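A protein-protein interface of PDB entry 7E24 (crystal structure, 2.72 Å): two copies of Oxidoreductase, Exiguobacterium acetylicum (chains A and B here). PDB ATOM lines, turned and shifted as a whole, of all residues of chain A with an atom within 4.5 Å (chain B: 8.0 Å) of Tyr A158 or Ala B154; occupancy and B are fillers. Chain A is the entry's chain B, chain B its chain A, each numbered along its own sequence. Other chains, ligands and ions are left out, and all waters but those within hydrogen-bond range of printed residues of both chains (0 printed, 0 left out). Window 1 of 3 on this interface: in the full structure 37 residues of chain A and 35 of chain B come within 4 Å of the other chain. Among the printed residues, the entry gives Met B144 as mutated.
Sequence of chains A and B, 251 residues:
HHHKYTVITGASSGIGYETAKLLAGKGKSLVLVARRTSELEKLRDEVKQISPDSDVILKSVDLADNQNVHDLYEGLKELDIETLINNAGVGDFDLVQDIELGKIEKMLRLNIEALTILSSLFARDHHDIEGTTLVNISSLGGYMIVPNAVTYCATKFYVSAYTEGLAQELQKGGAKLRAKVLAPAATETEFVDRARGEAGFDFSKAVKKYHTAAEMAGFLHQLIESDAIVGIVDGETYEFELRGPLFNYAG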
ATOM      1  N   ILE A 112     -19.972 -24.179 -11.711  1.00  0.00           N
ATOM      2  CA  ILE A 112     -19.386 -22.857 -11.860  1.00  0.00           C
ATOM      3  C   ILE A 112     -19.212 -22.497 -13.329  1.00  0.00           C
ATOM      4  O   ILE A 112     -19.875 -21.598 -13.831  1.00  0.00           O
ATOM      5  CB  ILE A 112     -18.063 -22.741 -11.071  1.00  0.00           C
ATOM      6  CG1 ILE A 112     -18.360 -22.872  -9.587  1.00  0.00           C
ATOM      7  CG2 ILE A 112     -17.407 -21.421 -11.334  1.00  0.00           C
ATOM      8  CD1 ILE A 112     -17.201 -22.578  -8.753  1.00  0.00           C
ATOM      9  N   THR A 116     -21.192 -19.994 -15.839  1.00  0.00           N
ATOM     10  CA  THR A 116     -20.582 -18.698 -16.096  1.00  0.00           C
ATOM     11  C   THR A 116     -20.412 -18.468 -17.588  1.00  0.00           C
ATOM     12  O   THR A 116     -20.562 -17.340 -18.064  1.00  0.00           O
ATOM     13  CB  THR A 116     -19.253 -18.597 -15.353  1.00  0.00           C
ATOM     14  OG1 THR A 116     -19.528 -18.580 -13.959  1.00  0.00           O
ATOM     15  CG2 THR A 116     -18.508 -17.329 -15.707  1.00  0.00           C
ATOM     16  N   ALA A 154     -19.430 -23.829  -1.729  1.00  0.00           N
ATOM     17  CA  ALA A 154     -18.599 -22.765  -2.277  1.00  0.00           C
ATOM     18  C   ALA A 154     -18.913 -22.520  -3.756  1.00  0.00           C
ATOM     19  O   ALA A 154     -18.870 -21.372  -4.223  1.00  0.00           O
ATOM     20  CB  ALA A 154     -17.130 -23.113  -2.075  1.00  0.00           C
ATOM     21  N   THR A 155     -19.217 -23.586  -4.520  1.00  0.00           N
ATOM     22  CA  THR A 155     -19.724 -23.366  -5.872  1.00  0.00           C
ATOM     23  C   THR A 155     -21.020 -22.568  -5.836  1.00  0.00           C
ATOM     24  O   THR A 155     -21.263 -21.724  -6.702  1.00  0.00           O
ATOM     25  CB  THR A 155     -19.957 -24.685  -6.592  1.00  0.00           C
ATOM     26  OG1 THR A 155     -20.971 -25.442  -5.918  1.00  0.00           O
ATOM     27  CG2 THR A 155     -18.706 -25.483  -6.673  1.00  0.00           C
ATOM     28  N   LYS A 156     -21.852 -22.793  -4.824  1.00  0.00           N
ATOM     29  CA  LYS A 156     -23.102 -22.056  -4.761  1.00  0.00           C
ATOM     30  C   LYS A 156     -22.892 -20.625  -4.262  1.00  0.00           C
ATOM     31  O   LYS A 156     -23.563 -19.717  -4.758  1.00  0.00           O
ATOM     32  CB  LYS A 156     -24.109 -22.809  -3.896  1.00  0.00           C
ATOM     33  CG  LYS A 156     -24.571 -24.122  -4.502  1.00  0.00           C
ATOM     34  CD  LYS A 156     -24.932 -23.970  -5.967  1.00  0.00           C
ATOM     35  CE  LYS A 156     -25.633 -25.212  -6.463  1.00  0.00           C
ATOM     36  NZ  LYS A 156     -26.098 -25.039  -7.853  1.00  0.00           N
ATOM     37  N   PHE A 157     -21.948 -20.383  -3.333  1.00  0.00           N
ATOM     38  CA  PHE A 157     -21.584 -19.004  -2.990  1.00  0.00           C
ATOM     39  C   PHE A 157     -21.089 -18.250  -4.212  1.00  0.00           C
ATOM     40  O   PHE A 157     -21.314 -17.039  -4.337  1.00  0.00           O
ATOM     41  CB  PHE A 157     -20.504 -18.971  -1.912  1.00  0.00           C
ATOM     42  CG  PHE A 157     -21.035 -18.923  -0.521  1.00  0.00           C
ATOM     43  CD1 PHE A 157     -21.465 -20.077   0.097  1.00  0.00           C
ATOM     44  CD2 PHE A 157     -21.117 -17.726   0.163  1.00  0.00           C
ATOM     45  CE1 PHE A 157     -21.954 -20.047   1.378  1.00  0.00           C
ATOM     46  CE2 PHE A 157     -21.620 -17.681   1.449  1.00  0.00           C
ATOM     47  CZ  PHE A 157     -22.035 -18.848   2.061  1.00  0.00           C
ATOM     48  N   TYR A 158     -20.373 -18.942  -5.107  1.00  0.00           N
ATOM     49  CA  TYR A 158     -19.999 -18.333  -6.375  1.00  0.00           C
ATOM     50  C   TYR A 158     -21.235 -17.981  -7.174  1.00  0.00           C
ATOM     51  O   TYR A 158     -21.325 -16.897  -7.756  1.00  0.00           O
ATOM     52  CB  TYR A 158     -19.103 -19.274  -7.187  1.00  0.00           C
ATOM     53  CG  TYR A 158     -18.783 -18.742  -8.577  1.00  0.00           C
ATOM     54  CD1 TYR A 158     -19.701 -18.826  -9.622  1.00  0.00           C
ATOM     55  CD2 TYR A 158     -17.567 -18.152  -8.836  1.00  0.00           C
ATOM     56  CE1 TYR A 158     -19.418 -18.328 -10.852  1.00  0.00           C
ATOM     57  CE2 TYR A 158     -17.271 -17.660 -10.071  1.00  0.00           C
ATOM     58  CZ  TYR A 158     -18.196 -17.748 -11.072  1.00  0.00           C
ATOM     59  OH  TYR A 158     -17.876 -17.250 -12.304  1.00  0.00           O
ATOM     60  N   VAL A 159     -22.184 -18.910  -7.258  1.00  0.00           N
ATOM     61  CA  VAL A 159     -23.356 -18.673  -8.091  1.00  0.00           C
ATOM     62  C   VAL A 159     -24.164 -17.500  -7.544  1.00  0.00           C
ATOM     63  O   VAL A 159     -24.515 -16.572  -8.280  1.00  0.00           O
ATOM     64  CB  VAL A 159     -24.194 -19.958  -8.203  1.00  0.00           C
ATOM     65  CG1 VAL A 159     -25.491 -19.680  -8.923  1.00  0.00           C
ATOM     66  CG2 VAL A 159     -23.395 -21.056  -8.935  1.00  0.00           C
ATOM     67  N   SER A 160     -24.405 -17.488  -6.227  1.00  0.00           N
ATOM     68  CA  SER A 160     -25.155 -16.403  -5.598  1.00  0.00           C
ATOM     69  C   SER A 160     -24.461 -15.067  -5.761  1.00  0.00           C
ATOM     70  O   SER A 160     -25.109 -14.052  -6.016  1.00  0.00           O
ATOM     71  CB  SER A 160     -25.362 -16.694  -4.118  1.00  0.00           C
ATOM     72  OG  SER A 160     -26.287 -17.720  -3.933  1.00  0.00           O
ATOM     73  N   ALA A 161     -23.153 -15.033  -5.538  1.00  0.00           N
ATOM     74  CA  ALA A 161     -22.441 -13.770  -5.625  1.00  0.00           C
ATOM     75  C   ALA A 161     -22.325 -13.324  -7.071  1.00  0.00           C
ATOM     76  O   ALA A 161     -22.515 -12.141  -7.375  1.00  0.00           O
ATOM     77  CB  ALA A 161     -21.069 -13.892  -4.969  1.00  0.00           C
ATOM     78  N   TYR A 162     -22.051 -14.263  -7.982  1.00  0.00           N
ATOM     79  CA  TYR A 162     -21.983 -13.922  -9.397  1.00  0.00           C
ATOM     80  C   TYR A 162     -23.311 -13.345  -9.876  1.00  0.00           C
ATOM     81  O   TYR A 162     -23.354 -12.268 -10.472  1.00  0.00           O
ATOM     82  CB  TYR A 162     -21.580 -15.164 -10.208  1.00  0.00           C
ATOM     83  CG  TYR A 162     -21.494 -14.948 -11.697  1.00  0.00           C
ATOM     84  CD1 TYR A 162     -20.379 -14.368 -12.274  1.00  0.00           C
ATOM     85  CD2 TYR A 162     -22.539 -15.326 -12.525  1.00  0.00           C
ATOM     86  CE1 TYR A 162     -20.308 -14.169 -13.627  1.00  0.00           C
ATOM     87  CE2 TYR A 162     -22.480 -15.129 -13.886  1.00  0.00           C
ATOM     88  CZ  TYR A 162     -21.359 -14.549 -14.432  1.00  0.00           C
ATOM     89  OH  TYR A 162     -21.269 -14.349 -15.782  1.00  0.00           O
ATOM     90  N   ILE B 104     -11.517 -15.115 -18.841  1.00  0.00           N
ATOM     91  CA  ILE B 104     -12.321 -15.364 -17.649  1.00  0.00           C
ATOM     92  C   ILE B 104     -12.301 -16.848 -17.298  1.00  0.00           C
ATOM     93  O   ILE B 104     -12.142 -17.216 -16.126  1.00  0.00           O
ATOM     94  CB  ILE B 104     -13.756 -14.838 -17.846  1.00  0.00           C
ATOM     95  CG1 ILE B 104     -13.903 -13.459 -17.220  1.00  0.00           C
ATOM     96  CG2 ILE B 104     -14.757 -15.761 -17.197  1.00  0.00           C
ATOM     97  CD1 ILE B 104     -12.916 -12.459 -17.750  1.00  0.00           C
ATOM     98  N   MET B 107      -9.190 -17.409 -15.676  1.00  0.00           N
ATOM     99  CA  MET B 107      -9.302 -16.913 -14.307  1.00  0.00           C
ATOM    100  C   MET B 107      -9.953 -17.942 -13.387  1.00  0.00           C
ATOM    101  O   MET B 107      -9.471 -18.189 -12.275  1.00  0.00           O
ATOM    102  CB  MET B 107     -10.085 -15.609 -14.272  1.00  0.00           C
ATOM    103  CG  MET B 107     -10.175 -15.041 -12.891  1.00  0.00           C
ATOM    104  SD  MET B 107     -11.051 -13.472 -12.818  1.00  0.00           S
ATOM    105  CE  MET B 107     -12.658 -13.871 -13.508  1.00  0.00           C
ATOM    106  N   LEU B 108     -11.043 -18.570 -13.831  1.00  0.00           N
ATOM    107  CA  LEU B 108     -11.686 -19.567 -12.982  1.00  0.00           C
ATOM    108  C   LEU B 108     -10.748 -20.739 -12.711  1.00  0.00           C
ATOM    109  O   LEU B 108     -10.694 -21.259 -11.592  1.00  0.00           O
ATOM    110  CB  LEU B 108     -12.976 -20.066 -13.623  1.00  0.00           C
ATOM    111  CG  LEU B 108     -14.056 -19.019 -13.912  1.00  0.00           C
ATOM    112  CD1 LEU B 108     -15.222 -19.679 -14.561  1.00  0.00           C
ATOM    113  CD2 LEU B 108     -14.488 -18.340 -12.652  1.00  0.00           C
ATOM    114  N   ASN B 111      -8.060 -19.064 -10.188  1.00  0.00           N
ATOM    115  CA  ASN B 111      -8.495 -18.537  -8.901  1.00  0.00           C
ATOM    116  C   ASN B 111      -9.201 -19.598  -8.073  1.00  0.00           C
ATOM    117  O   ASN B 111      -9.077 -19.614  -6.843  1.00  0.00           O
ATOM    118  CB  ASN B 111      -9.419 -17.340  -9.100  1.00  0.00           C
ATOM    119  CG  ASN B 111      -8.685 -16.109  -9.556  1.00  0.00           C
ATOM    120  OD1 ASN B 111      -7.569 -16.211 -10.086  1.00  0.00           O
ATOM    121  ND2 ASN B 111      -9.310 -14.946  -9.402  1.00  0.00           N
ATOM    122  N   ILE B 112      -9.915 -20.506  -8.719  1.00  0.00           N
ATOM    123  CA  ILE B 112     -10.808 -21.433  -8.045  1.00  0.00           C
ATOM    124  C   ILE B 112     -10.242 -22.842  -8.059  1.00  0.00           C
ATOM    125  O   ILE B 112     -10.106 -23.482  -7.015  1.00  0.00           O
ATOM    126  CB  ILE B 112     -12.215 -21.390  -8.677  1.00  0.00           C
ATOM    127  CG1 ILE B 112     -12.828 -20.011  -8.481  1.00  0.00           C
ATOM    128  CG2 ILE B 112     -13.074 -22.501  -8.088  1.00  0.00           C
ATOM    129  CD1 ILE B 112     -14.267 -19.970  -8.849  1.00  0.00           C
ATOM    130  N   GLY B 141     -13.035  -8.141  -1.926  1.00  0.00           N
ATOM    131  CA  GLY B 141     -13.959  -8.451  -2.994  1.00  0.00           C
ATOM    132  C   GLY B 141     -14.577  -9.820  -2.888  1.00  0.00           C
ATOM    133  O   GLY B 141     -15.526 -10.110  -3.629  1.00  0.00           O
ATOM    134  N   GLY B 142     -14.072 -10.667  -1.985  1.00  0.00           N
ATOM    135  CA  GLY B 142     -14.714 -11.939  -1.728  1.00  0.00           C
ATOM    136  C   GLY B 142     -15.720 -11.936  -0.605  1.00  0.00           C
ATOM    137  O   GLY B 142     -16.335 -12.972  -0.343  1.00  0.00           O
ATOM    138  N   MET B 144     -17.573  -8.692  -0.253  1.00  0.00           N
ATOM    139  CA  MET B 144     -18.381  -7.574  -0.714  1.00  0.00           C
ATOM    140  C   MET B 144     -18.239  -7.514  -2.228  1.00  0.00           C
ATOM    141  O   MET B 144     -17.114  -7.572  -2.729  1.00  0.00           O
ATOM    142  CB  MET B 144     -17.913  -6.271  -0.059  1.00  0.00           C
ATOM    143  CG  MET B 144     -18.145  -5.018  -0.841  1.00  0.00           C
ATOM    144  SD  MET B 144     -17.861  -3.611   0.234  1.00  0.00           S
ATOM    145  CE  MET B 144     -16.084  -3.721   0.466  1.00  0.00           C
ATOM    146  N   ILE B 145     -19.352  -7.385  -2.954  1.00  0.00           N
ATOM    147  CA  ILE B 145     -19.302  -7.364  -4.417  1.00  0.00           C
ATOM    148  C   ILE B 145     -18.910  -5.970  -4.894  1.00  0.00           C
ATOM    149  O   ILE B 145     -19.335  -4.968  -4.323  1.00  0.00           O
ATOM    150  CB  ILE B 145     -20.653  -7.822  -4.992  1.00  0.00           C
ATOM    151  CG1 ILE B 145     -20.860  -9.304  -4.671  1.00  0.00           C
ATOM    152  CG2 ILE B 145     -20.739  -7.593  -6.488  1.00  0.00           C
ATOM    153  CD1 ILE B 145     -22.278  -9.756  -4.814  1.00  0.00           C
ATOM    154  N   VAL B 146     -18.062  -5.890  -5.912  1.00  0.00           N
ATOM    155  CA  VAL B 146     -17.508  -4.626  -6.377  1.00  0.00           C
ATOM    156  C   VAL B 146     -17.951  -4.392  -7.818  1.00  0.00           C
ATOM    157  O   VAL B 146     -17.737  -5.262  -8.673  1.00  0.00           O
ATOM    158  CB  VAL B 146     -15.975  -4.625  -6.277  1.00  0.00           C
ATOM    159  CG1 VAL B 146     -15.411  -3.225  -6.517  1.00  0.00           C
ATOM    160  CG2 VAL B 146     -15.513  -5.175  -4.924  1.00  0.00           C
ATOM    161  N   ALA B 149     -16.442  -5.715 -11.541  1.00  0.00           N
ATOM    162  CA  ALA B 149     -15.570  -6.860 -11.295  1.00  0.00           C
ATOM    163  C   ALA B 149     -16.386  -8.023 -10.744  1.00  0.00           C
ATOM    164  O   ALA B 149     -15.958  -8.715  -9.816  1.00  0.00           O
ATOM    165  CB  ALA B 149     -14.424  -6.509 -10.339  1.00  0.00           C
ATOM    166  N   VAL B 150     -17.561  -8.258 -11.323  1.00  0.00           N
ATOM    167  CA  VAL B 150     -18.484  -9.258 -10.788  1.00  0.00           C
ATOM    168  C   VAL B 150     -17.857 -10.649 -10.821  1.00  0.00           C
ATOM    169  O   VAL B 150     -17.826 -11.362  -9.808  1.00  0.00           O
ATOM    170  CB  VAL B 150     -19.810  -9.230 -11.568  1.00  0.00           C
ATOM    171  CG1 VAL B 150     -20.735 -10.300 -11.056  1.00  0.00           C
ATOM    172  CG2 VAL B 150     -20.435  -7.875 -11.473  1.00  0.00           C
ATOM    173  N   THR B 151     -17.348 -11.055 -11.984  1.00  0.00           N
ATOM    174  CA  THR B 151     -16.846 -12.417 -12.142  1.00  0.00           C
ATOM    175  C   THR B 151     -15.694 -12.707 -11.186  1.00  0.00           C
ATOM    176  O   THR B 151     -15.659 -13.763 -10.544  1.00  0.00           O
ATOM    177  CB  THR B 151     -16.415 -12.647 -13.585  1.00  0.00           C
ATOM    178  OG1 THR B 151     -17.309 -11.950 -14.464  1.00  0.00           O
ATOM    179  CG2 THR B 151     -16.415 -14.128 -13.887  1.00  0.00           C
ATOM    180  N   TYR B 152     -14.741 -11.777 -11.071  1.00  0.00           N
ATOM    181  CA  TYR B 152     -13.599 -11.987 -10.179  1.00  0.00           C
ATOM    182  C   TYR B 152     -14.042 -12.030  -8.719  1.00  0.00           C
ATOM    183  O   TYR B 152     -13.556 -12.854  -7.932  1.00  0.00           O
ATOM    184  CB  TYR B 152     -12.568 -10.879 -10.386  1.00  0.00           C
ATOM    185  CG  TYR B 152     -11.600 -10.689  -9.249  1.00  0.00           C
ATOM    186  CD1 TYR B 152     -10.455 -11.465  -9.138  1.00  0.00           C
ATOM    187  CD2 TYR B 152     -11.825  -9.727  -8.289  1.00  0.00           C
ATOM    188  CE1 TYR B 152      -9.568 -11.272  -8.113  1.00  0.00           C
ATOM    189  CE2 TYR B 152     -10.953  -9.546  -7.265  1.00  0.00           C
ATOM    190  CZ  TYR B 152      -9.819 -10.316  -7.173  1.00  0.00           C
ATOM    191  OH  TYR B 152      -8.934 -10.117  -6.126  1.00  0.00           O
ATOM    192  N   CYS B 153     -14.967 -11.136  -8.337  1.00  0.00           N
ATOM    193  CA  CYS B 153     -15.479 -11.131  -6.973  1.00  0.00           C
ATOM    194  C   CYS B 153     -16.047 -12.492  -6.635  1.00  0.00           C
ATOM    195  O   CYS B 153     -15.805 -13.029  -5.552  1.00  0.00           O
ATOM    196  CB  CYS B 153     -16.539 -10.052  -6.818  1.00  0.00           C
ATOM    197  SG  CYS B 153     -15.833  -8.391  -6.775  1.00  0.00           S
ATOM    198  N   ALA B 154     -16.762 -13.093  -7.588  1.00  0.00           N
ATOM    199  CA  ALA B 154     -17.395 -14.378  -7.339  1.00  0.00           C
ATOM    200  C   ALA B 154     -16.350 -15.478  -7.159  1.00  0.00           C
ATOM    201  O   ALA B 154     -16.578 -16.439  -6.415  1.00  0.00           O
ATOM    202  CB  ALA B 154     -18.355 -14.699  -8.482  1.00  0.00           C
ATOM    203  N   THR B 155     -15.194 -15.376  -7.829  1.00  0.00           N
ATOM    204  CA  THR B 155     -14.146 -16.352  -7.542  1.00  0.00           C
ATOM    205  C   THR B 155     -13.643 -16.186  -6.110  1.00  0.00           C
ATOM    206  O   THR B 155     -13.354 -17.173  -5.431  1.00  0.00           O
ATOM    207  CB  THR B 155     -12.990 -16.245  -8.545  1.00  0.00           C
ATOM    208  OG1 THR B 155     -12.360 -14.962  -8.461  1.00  0.00           O
ATOM    209  CG2 THR B 155     -13.467 -16.462  -9.933  1.00  0.00           C
ATOM    210  N   LYS B 156     -13.597 -14.945  -5.608  1.00  0.00           N
ATOM    211  CA  LYS B 156     -13.137 -14.727  -4.239  1.00  0.00           C
ATOM    212  C   LYS B 156     -14.218 -15.060  -3.221  1.00  0.00           C
ATOM    213  O   LYS B 156     -13.889 -15.415  -2.079  1.00  0.00           O
ATOM    214  CB  LYS B 156     -12.682 -13.283  -4.037  1.00  0.00           C
ATOM    215  CG  LYS B 156     -11.482 -12.906  -4.868  1.00  0.00           C
ATOM    216  CD  LYS B 156     -10.400 -13.989  -4.806  1.00  0.00           C
ATOM    217  CE  LYS B 156      -9.145 -13.511  -5.514  1.00  0.00           C
ATOM    218  NZ  LYS B 156      -7.931 -14.245  -5.129  1.00  0.00           N
ATOM    219  N   PHE B 157     -15.505 -14.946  -3.592  1.00  0.00           N
ATOM    220  CA  PHE B 157     -16.550 -15.456  -2.714  1.00  0.00           C
ATOM    221  C   PHE B 157     -16.404 -16.952  -2.548  1.00  0.00           C
ATOM    222  O   PHE B 157     -16.493 -17.474  -1.430  1.00  0.00           O
ATOM    223  CB  PHE B 157     -17.924 -15.106  -3.253  1.00  0.00           C
ATOM    224  CG  PHE B 157     -18.478 -13.834  -2.695  1.00  0.00           C
ATOM    225  CD1 PHE B 157     -18.015 -12.616  -3.149  1.00  0.00           C
ATOM    226  CD2 PHE B 157     -19.447 -13.854  -1.700  1.00  0.00           C
ATOM    227  CE1 PHE B 157     -18.524 -11.439  -2.640  1.00  0.00           C
ATOM    228  CE2 PHE B 157     -19.950 -12.678  -1.185  1.00  0.00           C
ATOM    229  CZ  PHE B 157     -19.489 -11.470  -1.655  1.00  0.00           C
ATOM    230  N   TYR B 158     -16.138 -17.652  -3.654  1.00  0.00           N
ATOM    231  CA  TYR B 158     -15.806 -19.067  -3.591  1.00  0.00           C
ATOM    232  C   TYR B 158     -14.669 -19.299  -2.610  1.00  0.00           C
ATOM    233  O   TYR B 158     -14.792 -20.089  -1.668  1.00  0.00           O
ATOM    234  CB  TYR B 158     -15.435 -19.586  -4.984  1.00  0.00           C
ATOM    235  CG  TYR B 158     -15.042 -21.046  -4.953  1.00  0.00           C
ATOM    236  CD1 TYR B 158     -13.768 -21.445  -4.526  1.00  0.00           C
ATOM    237  CD2 TYR B 158     -15.949 -22.032  -5.316  1.00  0.00           C
ATOM    238  CE1 TYR B 158     -13.424 -22.758  -4.461  1.00  0.00           C
ATOM    239  CE2 TYR B 158     -15.601 -23.359  -5.263  1.00  0.00           C
ATOM    240  CZ  TYR B 158     -14.339 -23.706  -4.834  1.00  0.00           C
ATOM    241  OH  TYR B 158     -13.990 -25.015  -4.763  1.00  0.00           O
ATOM    242  N   VAL B 159     -13.545 -18.610  -2.827  1.00  0.00           N
ATOM    243  CA  VAL B 159     -12.359 -18.795  -1.994  1.00  0.00           C
ATOM    244  C   VAL B 159     -12.679 -18.537  -0.531  1.00  0.00           C
ATOM    245  O   VAL B 159     -12.275 -19.313   0.343  1.00  0.00           O
ATOM    246  CB  VAL B 159     -11.213 -17.895  -2.483  1.00  0.00           C
ATOM    247  CG1 VAL B 159     -10.049 -17.952  -1.521  1.00  0.00           C
ATOM    248  CG2 VAL B 159     -10.774 -18.309  -3.881  1.00  0.00           C
ATOM    249  N   SER B 160     -13.433 -17.466  -0.246  1.00  0.00           N
ATOM    250  CA  SER B 160     -13.759 -17.144   1.142  1.00  0.00           C
ATOM    251  C   SER B 160     -14.645 -18.205   1.756  1.00  0.00           C
ATOM    252  O   SER B 160     -14.421 -18.628   2.893  1.00  0.00           O
ATOM    253  CB  SER B 160     -14.446 -15.782   1.246  1.00  0.00           C
ATOM    254  OG  SER B 160     -13.521 -14.714   1.108  1.00  0.00           O
ATOM    255  N   ALA B 161     -15.675 -18.626   1.031  1.00  0.00           N
ATOM    256  CA  ALA B 161     -16.596 -19.597   1.595  1.00  0.00           C
ATOM    257  C   ALA B 161     -15.932 -20.960   1.706  1.00  0.00           C
ATOM    258  O   ALA B 161     -16.123 -21.673   2.695  1.00  0.00           O
ATOM    259  CB  ALA B 161     -17.860 -19.654   0.749  1.00  0.00           C
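Ile A112 touches Tyr B158, and with the chains exchanged Tyr A158 touches Ile B112. Ala A154 touches Tyr B158, and with the chains exchanged Tyr A158 touches Ala B154. Thr A155 touches Tyr B158, and with the chains exchanged Tyr A158 touches Thr B155. Phe A157 touches Ala B161, and with the chains exchanged Ala A161 touches Phe B157.
Among the printed residues, pairs that only touch across the chains: Ile A112 with Ile B112 (3.9 Å), Ile A112 with Tyr B158 (3.7 Å), Ala A154 with Tyr B158 (3.2 Å), Thr A155 with Tyr B158 (3.7 Å), Phe A157 with Ala B161 (3.5 Å), Tyr A158 with Leu B108 (3.6 Å), Tyr A158 with Ile B112 (3.8 Å), Tyr A158 with Thr B151 (3.8 Å), Tyr A158 with Ala B154 (3.1 Å), Tyr A158 with Thr B155 (3.8 Å), Ala A161 with Ile B145 (3.5 Å), Ala A161 with Phe B157 (3.4 Å), Tyr A162 with Val B150 (3.3 Å), Tyr A162 with Thr B151 (3.8 Å) and Tyr A162 with Ala B154 (3.7 Å).
ND2 of Asn B111 sits at hydrogen-bond distance from OG1 of Thr B155, at 3.2 Å. The backbone carbonyl oxygen (O) of Tyr B152 is in hydrogen-bond range of the side-chain hydroxyl (OG1) of Thr B155 (2.5 Å). O of Ile A112 is in hydrogen-bond range of OG1 of Thr A116, at 3.0 Å. The side-chain hydroxyl of Thr A116 is in hydrogen-bond range of the side-chain hydroxyl of Tyr A158 (2.7 Å).
Of the 11 printed residues of chain A, 7 touch a printed residue of chain B. Along chain A the printed residues that touch a printed residue of chain B span positions 112 to 162. Among the printed residues, 15 pairs touch across the chains. Among the printed residues, no Asp or Glu carboxylate lies within 4 Å of a Lys or Arg side-chain nitrogen of the other chain.
Of the printed residues of chain B, Ile A112 touches Ile B112 and Tyr B158. Tyr A158 touches just these residues of chain B: Leu B108 (3.6 Å), Ile B112 (3.8 Å), Thr B151 (3.8 Å), Ala B154 (3.1 Å) and Thr B155 (3.8 Å). Of the printed residues of chain B, Tyr A162 touches Val B150, Thr B151 and Ala B154. Of the printed residues of chain A, Ile B112 touches Ile A112 and Tyr A158. Gly B141 touches none of the printed residues of chain A. Printed residues of chain A within 4 Å of Thr B151: Tyr A158 (3.8 Å) and Tyr A162 (3.8 Å). Ala B154 touches two residues of chain A. Of the printed residues of chain A, Phe B157 touches Ala A161. Ser B160 touches none of the printed residues of chain A. The nearest residue of chain B that does not touch Tyr A158 is Tyr B158 (4.3 Å). The nearest residue of chain A that does not touch Ala B154 is Ala A161 (4.4 Å).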
